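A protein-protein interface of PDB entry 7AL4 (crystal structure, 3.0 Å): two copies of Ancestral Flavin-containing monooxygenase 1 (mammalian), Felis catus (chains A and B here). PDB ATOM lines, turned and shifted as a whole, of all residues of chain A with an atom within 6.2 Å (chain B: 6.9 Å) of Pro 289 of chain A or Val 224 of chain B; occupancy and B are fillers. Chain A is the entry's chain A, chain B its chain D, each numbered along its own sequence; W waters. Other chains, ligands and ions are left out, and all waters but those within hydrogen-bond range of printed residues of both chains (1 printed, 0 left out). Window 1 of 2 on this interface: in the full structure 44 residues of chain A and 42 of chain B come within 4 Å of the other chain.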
ATOM      1  N   VAL A 220      -4.047  33.190  20.455  1.00  0.00           N
ATOM      2  CA  VAL A 220      -3.364  32.226  21.367  1.00  0.00           C
ATOM      3  C   VAL A 220      -2.339  31.446  20.543  1.00  0.00           C
ATOM      4  O   VAL A 220      -2.712  30.949  19.458  1.00  0.00           O
ATOM      5  CB  VAL A 220      -4.377  31.281  22.041  1.00  0.00           C
ATOM      6  CG1 VAL A 220      -3.718  30.392  23.077  1.00  0.00           C
ATOM      7  CG2 VAL A 220      -5.541  32.035  22.657  1.00  0.00           C
ATOM      8  N   TRP A 263      -3.023  26.787  13.775  1.00  0.00           N
ATOM      9  CA  TRP A 263      -2.977  25.853  14.937  1.00  0.00           C
ATOM     10  C   TRP A 263      -4.372  25.279  15.179  1.00  0.00           C
ATOM     11  O   TRP A 263      -4.509  24.036  15.200  1.00  0.00           O
ATOM     12  CB  TRP A 263      -2.442  26.535  16.199  1.00  0.00           C
ATOM     13  CG  TRP A 263      -2.282  25.610  17.367  1.00  0.00           C
ATOM     14  CD1 TRP A 263      -2.174  24.249  17.340  1.00  0.00           C
ATOM     15  CD2 TRP A 263      -2.179  25.988  18.751  1.00  0.00           C
ATOM     16  NE1 TRP A 263      -2.031  23.756  18.608  1.00  0.00           N
ATOM     17  CE2 TRP A 263      -2.026  24.798  19.494  1.00  0.00           C
ATOM     18  CE3 TRP A 263      -2.208  27.210  19.431  1.00  0.00           C
ATOM     19  CZ2 TRP A 263      -1.899  24.802  20.883  1.00  0.00           C
ATOM     20  CZ3 TRP A 263      -2.085  27.211  20.803  1.00  0.00           C
ATOM     21  CH2 TRP A 263      -1.929  26.023  21.517  1.00  0.00           C
ATOM     22  N   PHE A 264      -5.352  26.165  15.368  1.00  0.00           N
ATOM     23  CA  PHE A 264      -6.785  25.812  15.564  1.00  0.00           C
ATOM     24  C   PHE A 264      -7.668  27.020  15.226  1.00  0.00           C
ATOM     25  O   PHE A 264      -7.297  28.158  15.618  1.00  0.00           O
ATOM     26  CB  PHE A 264      -7.027  25.353  17.003  1.00  0.00           C
ATOM     27  CG  PHE A 264      -6.929  26.468  18.012  1.00  0.00           C
ATOM     28  CD1 PHE A 264      -8.066  27.145  18.415  1.00  0.00           C
ATOM     29  CD2 PHE A 264      -5.705  26.864  18.527  1.00  0.00           C
ATOM     30  CE1 PHE A 264      -7.983  28.179  19.331  1.00  0.00           C
ATOM     31  CE2 PHE A 264      -5.625  27.893  19.450  1.00  0.00           C
ATOM     32  CZ  PHE A 264      -6.765  28.549  19.851  1.00  0.00           C
ATOM     33  N   TYR A 269     -13.543  27.909  18.454  1.00  0.00           N
ATOM     34  CA  TYR A 269     -13.185  27.783  19.897  1.00  0.00           C
ATOM     35  C   TYR A 269     -13.747  28.965  20.698  1.00  0.00           C
ATOM     36  O   TYR A 269     -13.816  28.874  21.945  1.00  0.00           O
ATOM     37  CB  TYR A 269     -11.673  27.644  20.054  1.00  0.00           C
ATOM     38  CG  TYR A 269     -11.175  26.259  19.741  1.00  0.00           C
ATOM     39  CD1 TYR A 269     -10.464  25.526  20.673  1.00  0.00           C
ATOM     40  CD2 TYR A 269     -11.465  25.652  18.530  1.00  0.00           C
ATOM     41  CE1 TYR A 269     -10.024  24.241  20.401  1.00  0.00           C
ATOM     42  CE2 TYR A 269     -11.035  24.369  18.242  1.00  0.00           C
ATOM     43  CZ  TYR A 269     -10.308  23.658  19.178  1.00  0.00           C
ATOM     44  OH  TYR A 269      -9.881  22.394  18.879  1.00  0.00           O
ATOM     45  N   LEU A 271     -12.573  32.168  20.614  1.00  0.00           N
ATOM     46  CA  LEU A 271     -11.458  33.033  21.081  1.00  0.00           C
ATOM     47  C   LEU A 271     -11.386  34.285  20.206  1.00  0.00           C
ATOM     48  O   LEU A 271     -11.093  35.362  20.753  1.00  0.00           O
ATOM     49  CB  LEU A 271     -10.151  32.235  21.034  1.00  0.00           C
ATOM     50  CG  LEU A 271     -10.009  31.195  22.139  1.00  0.00           C
ATOM     51  CD1 LEU A 271      -8.893  30.214  21.843  1.00  0.00           C
ATOM     52  CD2 LEU A 271      -9.785  31.866  23.482  1.00  0.00           C
ATOM     53  N   ASN A 285       0.040  30.091  25.805  1.00  0.00           N
ATOM     54  CA  ASN A 285      -0.355  28.859  26.531  1.00  0.00           C
ATOM     55  C   ASN A 285      -0.303  27.695  25.542  1.00  0.00           C
ATOM     56  O   ASN A 285      -0.712  27.890  24.399  1.00  0.00           O
ATOM     57  CB  ASN A 285      -1.721  29.028  27.191  1.00  0.00           C
ATOM     58  CG  ASN A 285      -1.920  28.050  28.322  1.00  0.00           C
ATOM     59  OD1 ASN A 285      -1.845  26.840  28.118  1.00  0.00           O
ATOM     60  ND2 ASN A 285      -2.143  28.570  29.518  1.00  0.00           N
ATOM     61  N   ASP A 286       0.236  26.553  25.958  1.00  0.00           N
ATOM     62  CA  ASP A 286       0.369  25.353  25.088  1.00  0.00           C
ATOM     63  C   ASP A 286      -0.768  24.369  25.353  1.00  0.00           C
ATOM     64  O   ASP A 286      -0.922  23.433  24.547  1.00  0.00           O
ATOM     65  CB  ASP A 286       1.669  24.601  25.343  1.00  0.00           C
ATOM     66  CG  ASP A 286       2.848  25.519  25.518  1.00  0.00           C
ATOM     67  OD1 ASP A 286       2.994  26.426  24.681  1.00  0.00           O
ATOM     68  OD2 ASP A 286       3.588  25.327  26.499  1.00  0.00           O
ATOM     69  N   GLU A 287      -1.499  24.553  26.455  1.00  0.00           N
ATOM     70  CA  GLU A 287      -2.522  23.578  26.921  1.00  0.00           C
ATOM     71  C   GLU A 287      -3.902  23.978  26.384  1.00  0.00           C
ATOM     72  O   GLU A 287      -4.582  23.087  25.832  1.00  0.00           O
ATOM     73  CB  GLU A 287      -2.488  23.475  28.447  1.00  0.00           C
ATOM     74  CG  GLU A 287      -1.186  22.906  28.997  1.00  0.00           C
ATOM     75  CD  GLU A 287      -1.184  22.618  30.496  1.00  0.00           C
ATOM     76  OE1 GLU A 287      -2.201  22.108  31.013  1.00  0.00           O
ATOM     77  OE2 GLU A 287      -0.164  22.913  31.154  1.00  0.00           O
ATOM     78  N   LEU A 288      -4.248  25.269  26.485  1.00  0.00           N
ATOM     79  CA  LEU A 288      -5.644  25.790  26.382  1.00  0.00           C
ATOM     80  C   LEU A 288      -6.471  24.957  25.408  1.00  0.00           C
ATOM     81  O   LEU A 288      -7.447  24.341  25.819  1.00  0.00           O
ATOM     82  CB  LEU A 288      -5.651  27.259  25.953  1.00  0.00           C
ATOM     83  CG  LEU A 288      -6.747  28.132  26.567  1.00  0.00           C
ATOM     84  CD1 LEU A 288      -7.124  29.264  25.622  1.00  0.00           C
ATOM     85  CD2 LEU A 288      -7.984  27.338  26.946  1.00  0.00           C
ATOM     86  N   PRO A 289      -6.129  24.896  24.103  1.00  0.00           N
ATOM     87  CA  PRO A 289      -6.990  24.219  23.127  1.00  0.00           C
ATOM     88  C   PRO A 289      -7.343  22.778  23.529  1.00  0.00           C
ATOM     89  O   PRO A 289      -8.525  22.421  23.510  1.00  0.00           O
ATOM     90  CB  PRO A 289      -6.147  24.254  21.852  1.00  0.00           C
ATOM     91  CG  PRO A 289      -5.301  25.490  22.037  1.00  0.00           C
ATOM     92  CD  PRO A 289      -4.902  25.432  23.494  1.00  0.00           C
ATOM     93  N   GLY A 290      -6.327  22.009  23.927  1.00  0.00           N
ATOM     94  CA  GLY A 290      -6.488  20.671  24.541  1.00  0.00           C
ATOM     95  C   GLY A 290      -7.572  20.645  25.613  1.00  0.00           C
ATOM     96  O   GLY A 290      -8.296  19.637  25.692  1.00  0.00           O
ATOM     97  N   CYS A 291      -7.678  21.711  26.418  1.00  0.00           N
ATOM     98  CA  CYS A 291      -8.719  21.886  27.474  1.00  0.00           C
ATOM     99  C   CYS A 291     -10.079  22.182  26.846  1.00  0.00           C
ATOM    100  O   CYS A 291     -11.095  21.632  27.347  1.00  0.00           O
ATOM    101  CB  CYS A 291      -8.440  23.050  28.417  1.00  0.00           C
ATOM    102  SG  CYS A 291      -6.841  22.967  29.245  1.00  0.00           S
ATOM    103  N   ILE A 292     -10.101  23.058  25.838  1.00  0.00           N
ATOM    104  CA  ILE A 292     -11.372  23.516  25.204  1.00  0.00           C
ATOM    105  C   ILE A 292     -12.006  22.311  24.510  1.00  0.00           C
ATOM    106  O   ILE A 292     -13.213  22.070  24.729  1.00  0.00           O
ATOM    107  CB  ILE A 292     -11.153  24.689  24.234  1.00  0.00           C
ATOM    108  CG1 ILE A 292     -10.481  25.878  24.920  1.00  0.00           C
ATOM    109  CG2 ILE A 292     -12.470  25.110  23.599  1.00  0.00           C
ATOM    110  CD1 ILE A 292      -9.837  26.858  23.957  1.00  0.00           C
ATOM    111  N   ILE A 293     -11.208  21.572  23.737  1.00  0.00           N
ATOM    112  CA  ILE A 293     -11.717  20.451  22.900  1.00  0.00           C
ATOM    113  C   ILE A 293     -12.168  19.302  23.802  1.00  0.00           C
ATOM    114  O   ILE A 293     -13.067  18.545  23.367  1.00  0.00           O
ATOM    115  CB  ILE A 293     -10.669  19.996  21.877  1.00  0.00           C
ATOM    116  CG1 ILE A 293     -11.325  19.211  20.737  1.00  0.00           C
ATOM    117  CG2 ILE A 293      -9.567  19.206  22.552  1.00  0.00           C
ATOM    118  CD1 ILE A 293     -10.652  19.389  19.395  1.00  0.00           C
ATOM    119  N   THR A 294     -11.582  19.187  24.996  1.00  0.00           N
ATOM    120  CA  THR A 294     -11.963  18.178  26.029  1.00  0.00           C
ATOM    121  C   THR A 294     -12.955  18.775  27.040  1.00  0.00           C
ATOM    122  O   THR A 294     -13.456  18.025  27.911  1.00  0.00           O
ATOM    123  CB  THR A 294     -10.723  17.618  26.728  1.00  0.00           C
ATOM    124  OG1 THR A 294     -10.017  18.711  27.314  1.00  0.00           O
ATOM    125  CG2 THR A 294      -9.824  16.870  25.774  1.00  0.00           C
ATOM    126  N   TYR B  81     -14.296  15.742  22.731  1.00  0.00           N
ATOM    127  CA  TYR B  81     -13.643  14.553  23.342  1.00  0.00           C
ATOM    128  C   TYR B  81     -14.081  14.425  24.803  1.00  0.00           C
ATOM    129  O   TYR B  81     -13.723  15.269  25.640  1.00  0.00           O
ATOM    130  CB  TYR B  81     -12.129  14.632  23.225  1.00  0.00           C
ATOM    131  CG  TYR B  81     -11.606  14.531  21.818  1.00  0.00           C
ATOM    132  CD1 TYR B  81     -11.136  13.336  21.308  1.00  0.00           C
ATOM    133  CD2 TYR B  81     -11.533  15.649  21.009  1.00  0.00           C
ATOM    134  CE1 TYR B  81     -10.616  13.250  20.027  1.00  0.00           C
ATOM    135  CE2 TYR B  81     -11.023  15.583  19.723  1.00  0.00           C
ATOM    136  CZ  TYR B  81     -10.566  14.376  19.227  1.00  0.00           C
ATOM    137  OH  TYR B  81     -10.065  14.301  17.959  1.00  0.00           O
ATOM    138  N   MET B 221       0.514  13.109  18.038  1.00  0.00           N
ATOM    139  CA  MET B 221      -0.405  14.095  17.414  1.00  0.00           C
ATOM    140  C   MET B 221      -1.421  14.565  18.450  1.00  0.00           C
ATOM    141  O   MET B 221      -1.691  13.828  19.417  1.00  0.00           O
ATOM    142  CB  MET B 221      -1.154  13.520  16.205  1.00  0.00           C
ATOM    143  CG  MET B 221      -1.400  12.021  16.268  1.00  0.00           C
ATOM    144  SD  MET B 221      -2.832  11.496  15.299  1.00  0.00           S
ATOM    145  CE  MET B 221      -2.608  12.434  13.788  1.00  0.00           C
ATOM    146  N   SER B 222      -1.957  15.762  18.232  1.00  0.00           N
ATOM    147  CA  SER B 222      -2.958  16.425  19.108  1.00  0.00           C
ATOM    148  C   SER B 222      -4.377  16.023  18.679  1.00  0.00           C
ATOM    149  O   SER B 222      -4.583  15.690  17.488  1.00  0.00           O
ATOM    150  CB  SER B 222      -2.783  17.921  19.087  1.00  0.00           C
ATOM    151  OG  SER B 222      -3.930  18.562  19.597  1.00  0.00           O
ATOM    152  N   ARG B 223      -5.306  16.044  19.635  1.00  0.00           N
ATOM    153  CA  ARG B 223      -6.763  16.017  19.374  1.00  0.00           C
ATOM    154  C   ARG B 223      -7.118  17.224  18.511  1.00  0.00           C
ATOM    155  O   ARG B 223      -7.965  17.080  17.609  1.00  0.00           O
ATOM    156  CB  ARG B 223      -7.560  16.084  20.677  1.00  0.00           C
ATOM    157  CG  ARG B 223      -7.351  14.890  21.588  1.00  0.00           C
ATOM    158  CD  ARG B 223      -8.131  15.067  22.866  1.00  0.00           C
ATOM    159  NE  ARG B 223      -8.234  13.804  23.575  1.00  0.00           N
ATOM    160  CZ  ARG B 223      -7.269  13.264  24.316  1.00  0.00           C
ATOM    161  NH1 ARG B 223      -6.105  13.878  24.463  1.00  0.00           N
ATOM    162  NH2 ARG B 223      -7.476  12.105  24.919  1.00  0.00           N
ATOM    163  N   VAL B 224      -6.484  18.358  18.807  1.00  0.00           N
ATOM    164  CA  VAL B 224      -6.729  19.675  18.146  1.00  0.00           C
ATOM    165  C   VAL B 224      -6.586  19.509  16.628  1.00  0.00           C
ATOM    166  O   VAL B 224      -7.533  19.903  15.906  1.00  0.00           O
ATOM    167  CB  VAL B 224      -5.805  20.765  18.727  1.00  0.00           C
ATOM    168  CG1 VAL B 224      -5.009  21.531  17.671  1.00  0.00           C
ATOM    169  CG2 VAL B 224      -6.584  21.721  19.620  1.00  0.00           C
ATOM    170  N   PHE B 225      -5.457  18.955  16.170  1.00  0.00           N
ATOM    171  CA  PHE B 225      -5.167  18.644  14.740  1.00  0.00           C
ATOM    172  C   PHE B 225      -5.541  19.837  13.839  1.00  0.00           C
ATOM    173  O   PHE B 225      -5.392  20.993  14.278  1.00  0.00           O
ATOM    174  CB  PHE B 225      -5.883  17.349  14.338  1.00  0.00           C
ATOM    175  CG  PHE B 225      -5.190  16.553  13.258  1.00  0.00           C
ATOM    176  CD1 PHE B 225      -3.888  16.108  13.433  1.00  0.00           C
ATOM    177  CD2 PHE B 225      -5.841  16.234  12.073  1.00  0.00           C
ATOM    178  CE1 PHE B 225      -3.250  15.376  12.443  1.00  0.00           C
ATOM    179  CE2 PHE B 225      -5.203  15.493  11.089  1.00  0.00           C
ATOM    180  CZ  PHE B 225      -3.909  15.065  11.275  1.00  0.00           C
ATOM    181  N   ASP B 226      -5.998  19.575  12.610  1.00  0.00           N
ATOM    182  CA  ASP B 226      -6.089  20.593  11.529  1.00  0.00           C
ATOM    183  C   ASP B 226      -7.240  21.553  11.823  1.00  0.00           C
ATOM    184  O   ASP B 226      -8.399  21.108  11.764  1.00  0.00           O
ATOM    185  CB  ASP B 226      -6.278  19.937  10.161  1.00  0.00           C
ATOM    186  CG  ASP B 226      -5.124  19.050   9.727  1.00  0.00           C
ATOM    187  OD1 ASP B 226      -4.084  19.050  10.417  1.00  0.00           O
ATOM    188  OD2 ASP B 226      -5.279  18.368   8.698  1.00  0.00           O
ATOM    189  N   SER B 227      -6.912  22.810  12.130  1.00  0.00           N
ATOM    190  CA  SER B 227      -7.867  23.952  12.213  1.00  0.00           C
ATOM    191  C   SER B 227      -8.817  23.779  13.407  1.00  0.00           C
ATOM    192  O   SER B 227      -9.939  24.338  13.357  1.00  0.00           O
ATOM    193  CB  SER B 227      -8.647  24.092  10.921  1.00  0.00           C
ATOM    194  OG  SER B 227      -7.832  23.806   9.793  1.00  0.00           O
ATOM    195  N   GLY B 228      -8.381  23.051  14.442  1.00  0.00           N
ATOM    196  CA  GLY B 228      -9.193  22.739  15.640  1.00  0.00           C
ATOM    197  C   GLY B 228     -10.302  21.746  15.332  1.00  0.00           C
ATOM    198  O   GLY B 228     -11.389  21.813  15.967  1.00  0.00           O
ATOM    199  N   TYR B 229     -10.056  20.877  14.354  1.00  0.00           N
ATOM    200  CA  TYR B 229     -10.971  19.771  13.989  1.00  0.00           C
ATOM    201  C   TYR B 229     -10.466  18.518  14.675  1.00  0.00           C
ATOM    202  O   TYR B 229      -9.277  18.223  14.609  1.00  0.00           O
ATOM    203  CB  TYR B 229     -11.040  19.557  12.477  1.00  0.00           C
ATOM    204  CG  TYR B 229     -11.566  20.721  11.678  1.00  0.00           C
ATOM    205  CD1 TYR B 229     -12.312  21.731  12.262  1.00  0.00           C
ATOM    206  CD2 TYR B 229     -11.341  20.791  10.312  1.00  0.00           C
ATOM    207  CE1 TYR B 229     -12.792  22.793  11.515  1.00  0.00           C
ATOM    208  CE2 TYR B 229     -11.822  21.842   9.550  1.00  0.00           C
ATOM    209  CZ  TYR B 229     -12.551  22.845  10.154  1.00  0.00           C
ATOM    210  OH  TYR B 229     -13.034  23.881   9.412  1.00  0.00           O
ATOM    211  N   PRO B 230     -11.348  17.760  15.357  1.00  0.00           N
ATOM    212  CA  PRO B 230     -10.970  16.456  15.881  1.00  0.00           C
ATOM    213  C   PRO B 230     -10.238  15.688  14.775  1.00  0.00           C
ATOM    214  O   PRO B 230     -10.750  15.613  13.662  1.00  0.00           O
ATOM    215  CB  PRO B 230     -12.311  15.825  16.280  1.00  0.00           C
ATOM    216  CG  PRO B 230     -13.209  17.007  16.594  1.00  0.00           C
ATOM    217  CD  PRO B 230     -12.746  18.109  15.663  1.00  0.00           C
ATOM    218  N   TRP B 231      -9.036  15.209  15.095  1.00  0.00           N
ATOM    219  CA  TRP B 231      -8.125  14.553  14.118  1.00  0.00           C
ATOM    220  C   TRP B 231      -8.902  13.507  13.304  1.00  0.00           C
ATOM    221  O   TRP B 231      -8.786  13.519  12.063  1.00  0.00           O
ATOM    222  CB  TRP B 231      -6.909  13.942  14.821  1.00  0.00           C
ATOM    223  CG  TRP B 231      -7.267  12.810  15.723  1.00  0.00           C
ATOM    224  CD1 TRP B 231      -7.717  12.899  17.003  1.00  0.00           C
ATOM    225  CD2 TRP B 231      -7.264  11.414  15.393  1.00  0.00           C
ATOM    226  NE1 TRP B 231      -7.977  11.653  17.500  1.00  0.00           N
ATOM    227  CE2 TRP B 231      -7.713  10.718  16.534  1.00  0.00           C
ATOM    228  CE3 TRP B 231      -6.938  10.684  14.247  1.00  0.00           C
ATOM    229  CZ2 TRP B 231      -7.828   9.328  16.565  1.00  0.00           C
ATOM    230  CZ3 TRP B 231      -7.063   9.312  14.274  1.00  0.00           C
ATOM    231  CH2 TRP B 231      -7.495   8.645  15.420  1.00  0.00           C
ATOM    232  N   VAL B 234     -11.066  14.285  10.394  1.00  0.00           N
ATOM    233  CA  VAL B 234     -10.246  14.715   9.222  1.00  0.00           C
ATOM    234  C   VAL B 234      -9.584  13.478   8.611  1.00  0.00           C
ATOM    235  O   VAL B 234      -9.613  13.328   7.375  1.00  0.00           O
ATOM    236  CB  VAL B 234      -9.195  15.762   9.643  1.00  0.00           C
ATOM    237  CG1 VAL B 234      -8.359  16.231   8.460  1.00  0.00           C
ATOM    238  CG2 VAL B 234      -9.837  16.948  10.348  1.00  0.00           C
ATOM    239  N   LEU B 284      -1.667   9.903  21.289  1.00  0.00           N
ATOM    240  CA  LEU B 284      -2.624  11.043  21.266  1.00  0.00           C
ATOM    241  C   LEU B 284      -2.555  11.799  22.589  1.00  0.00           C
ATOM    242  O   LEU B 284      -3.225  11.387  23.569  1.00  0.00           O
ATOM    243  CB  LEU B 284      -4.039  10.537  20.978  1.00  0.00           C
ATOM    244  CG  LEU B 284      -4.454  10.703  19.521  1.00  0.00           C
ATOM    245  CD1 LEU B 284      -5.386   9.591  19.084  1.00  0.00           C
ATOM    246  CD2 LEU B 284      -5.075  12.072  19.300  1.00  0.00           C
ATOM    247  N   ASP B 286      -2.021  16.159  23.780  1.00  0.00           N
ATOM    248  CA  ASP B 286      -1.973  17.578  23.336  1.00  0.00           C
ATOM    249  C   ASP B 286      -0.916  18.347  24.128  1.00  0.00           C
ATOM    250  O   ASP B 286      -0.555  19.454  23.684  1.00  0.00           O
ATOM    251  CB  ASP B 286      -3.323  18.267  23.527  1.00  0.00           C
ATOM    252  CG  ASP B 286      -4.492  17.392  23.136  1.00  0.00           C
ATOM    253  OD1 ASP B 286      -4.397  16.770  22.063  1.00  0.00           O
ATOM    254  OD2 ASP B 286      -5.462  17.333  23.922  1.00  0.00           O
HETATM  255  O   HOH W   1      -6.396  17.082  26.834  1.00  0.00           O
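The backbone carbonyl oxygen (O) of Ile 293 of chain A sits at hydrogen-bond distance from the backbone NH (N) of Tyr 81 of chain B (3.1 Å). The backbone carbonyl oxygen (O) of Gly 228 of chain B sits close to the side-chain hydroxyl (OH) of Tyr 269 of chain A, at 3.3 Å. The backbone carbonyl oxygen (O) of Trp 263 of chain A sits close to the backbone carbonyl oxygen (O) of Phe 225 of chain B (3.3 Å).
OH of Tyr 81 of chain B lies close to N of Trp 231 of chain B (3.2 Å). The side-chain carboxylate of Asp 286 of chain B is in hydrogen-bond range of the side-chain hydroxyl of Ser 222 of chain B. O of Arg 223 of chain B sits at hydrogen-bond distance from N of Trp 231 of chain B (3.3 Å). The backbone carbonyl oxygen of Val 224 of chain B is in hydrogen-bond range of the backbone NH of Tyr 229 of chain B. OG1 of Thr 294 of chain A is in hydrogen-bond range of O of Gly 290 of chain A (2.5 Å). The backbone carbonyl oxygen of Cys 291 of chain A is in hydrogen-bond range of the side-chain hydroxyl of Thr 294 of chain A (3.1 Å).
CG1 of Val 224 of chain B touches O of Trp 263 of chain A, at 3.6 Å. C of Ser 227 of chain B touches CA of Phe 264 of chain A, 3.6 Å away. Gly 228 of chain B touches Phe 264 of chain A. Tyr 269 of chain A touches Val 224 of chain B (OH to CG2, 3.4 Å). Val 224 of chain B touches Pro 289 of chain A (CG2 to CB, 3.4 Å). CA of Gly 290 of chain A touches OD2 of Asp 286 of chain B, 3.5 Å away. O of Arg 223 of chain B touches CD1 of Ile 293 of chain A, 3.97 Å away. Tyr 81 of chain B touches Thr 294 of chain A. CG2 of Thr 294 of chain A touches CD of Arg 223 of chain B (3.8 Å).
Pro 289 of chain A touches one residue of chain B. Of the printed residues of chain B, Gly 290 of chain A touches Asp 286. Of the printed residues of chain B, Thr 294 of chain A touches Tyr 81 and Arg 223. Of the printed residues of chain A, Arg 223 of chain B touches Ile 293 (3.97 Å) and Thr 294 (3.8 Å). Of chain A, only Trp 263, Tyr 269 and Pro 289 come within 4 Å of Val 224 of chain B. The nearest residue of chain B that does not touch Pro 289 of chain A is Asp 286 of chain B (5.8 Å). The nearest printed residue of chain A that does not touch Arg 223 of chain B is Gly 290 of chain A (5.4 Å).
Hydrophobic or aromatic side chains of chain B that line the printed part of chain A: Tyr 81 and Val 224. Of the 15 printed residues of chain A, 7 touch a printed residue of chain B. Along chain A the printed residues that touch a printed residue of chain B span positions 263 to 294. Among the printed residues, no Asp or Glu carboxylate lies within 4 Å of a Lys or Arg side-chain nitrogen of the other chain.
Position printed for both chains: 286. Of the 12 pairs that touch across the chains among the printed residues, none has its exchanged pair printed and touching as well.
Water W1 bridges OD2 of Asp 286 of chain B (3.1 Å) and O of Gly 290 of chain A (3.4 Å).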
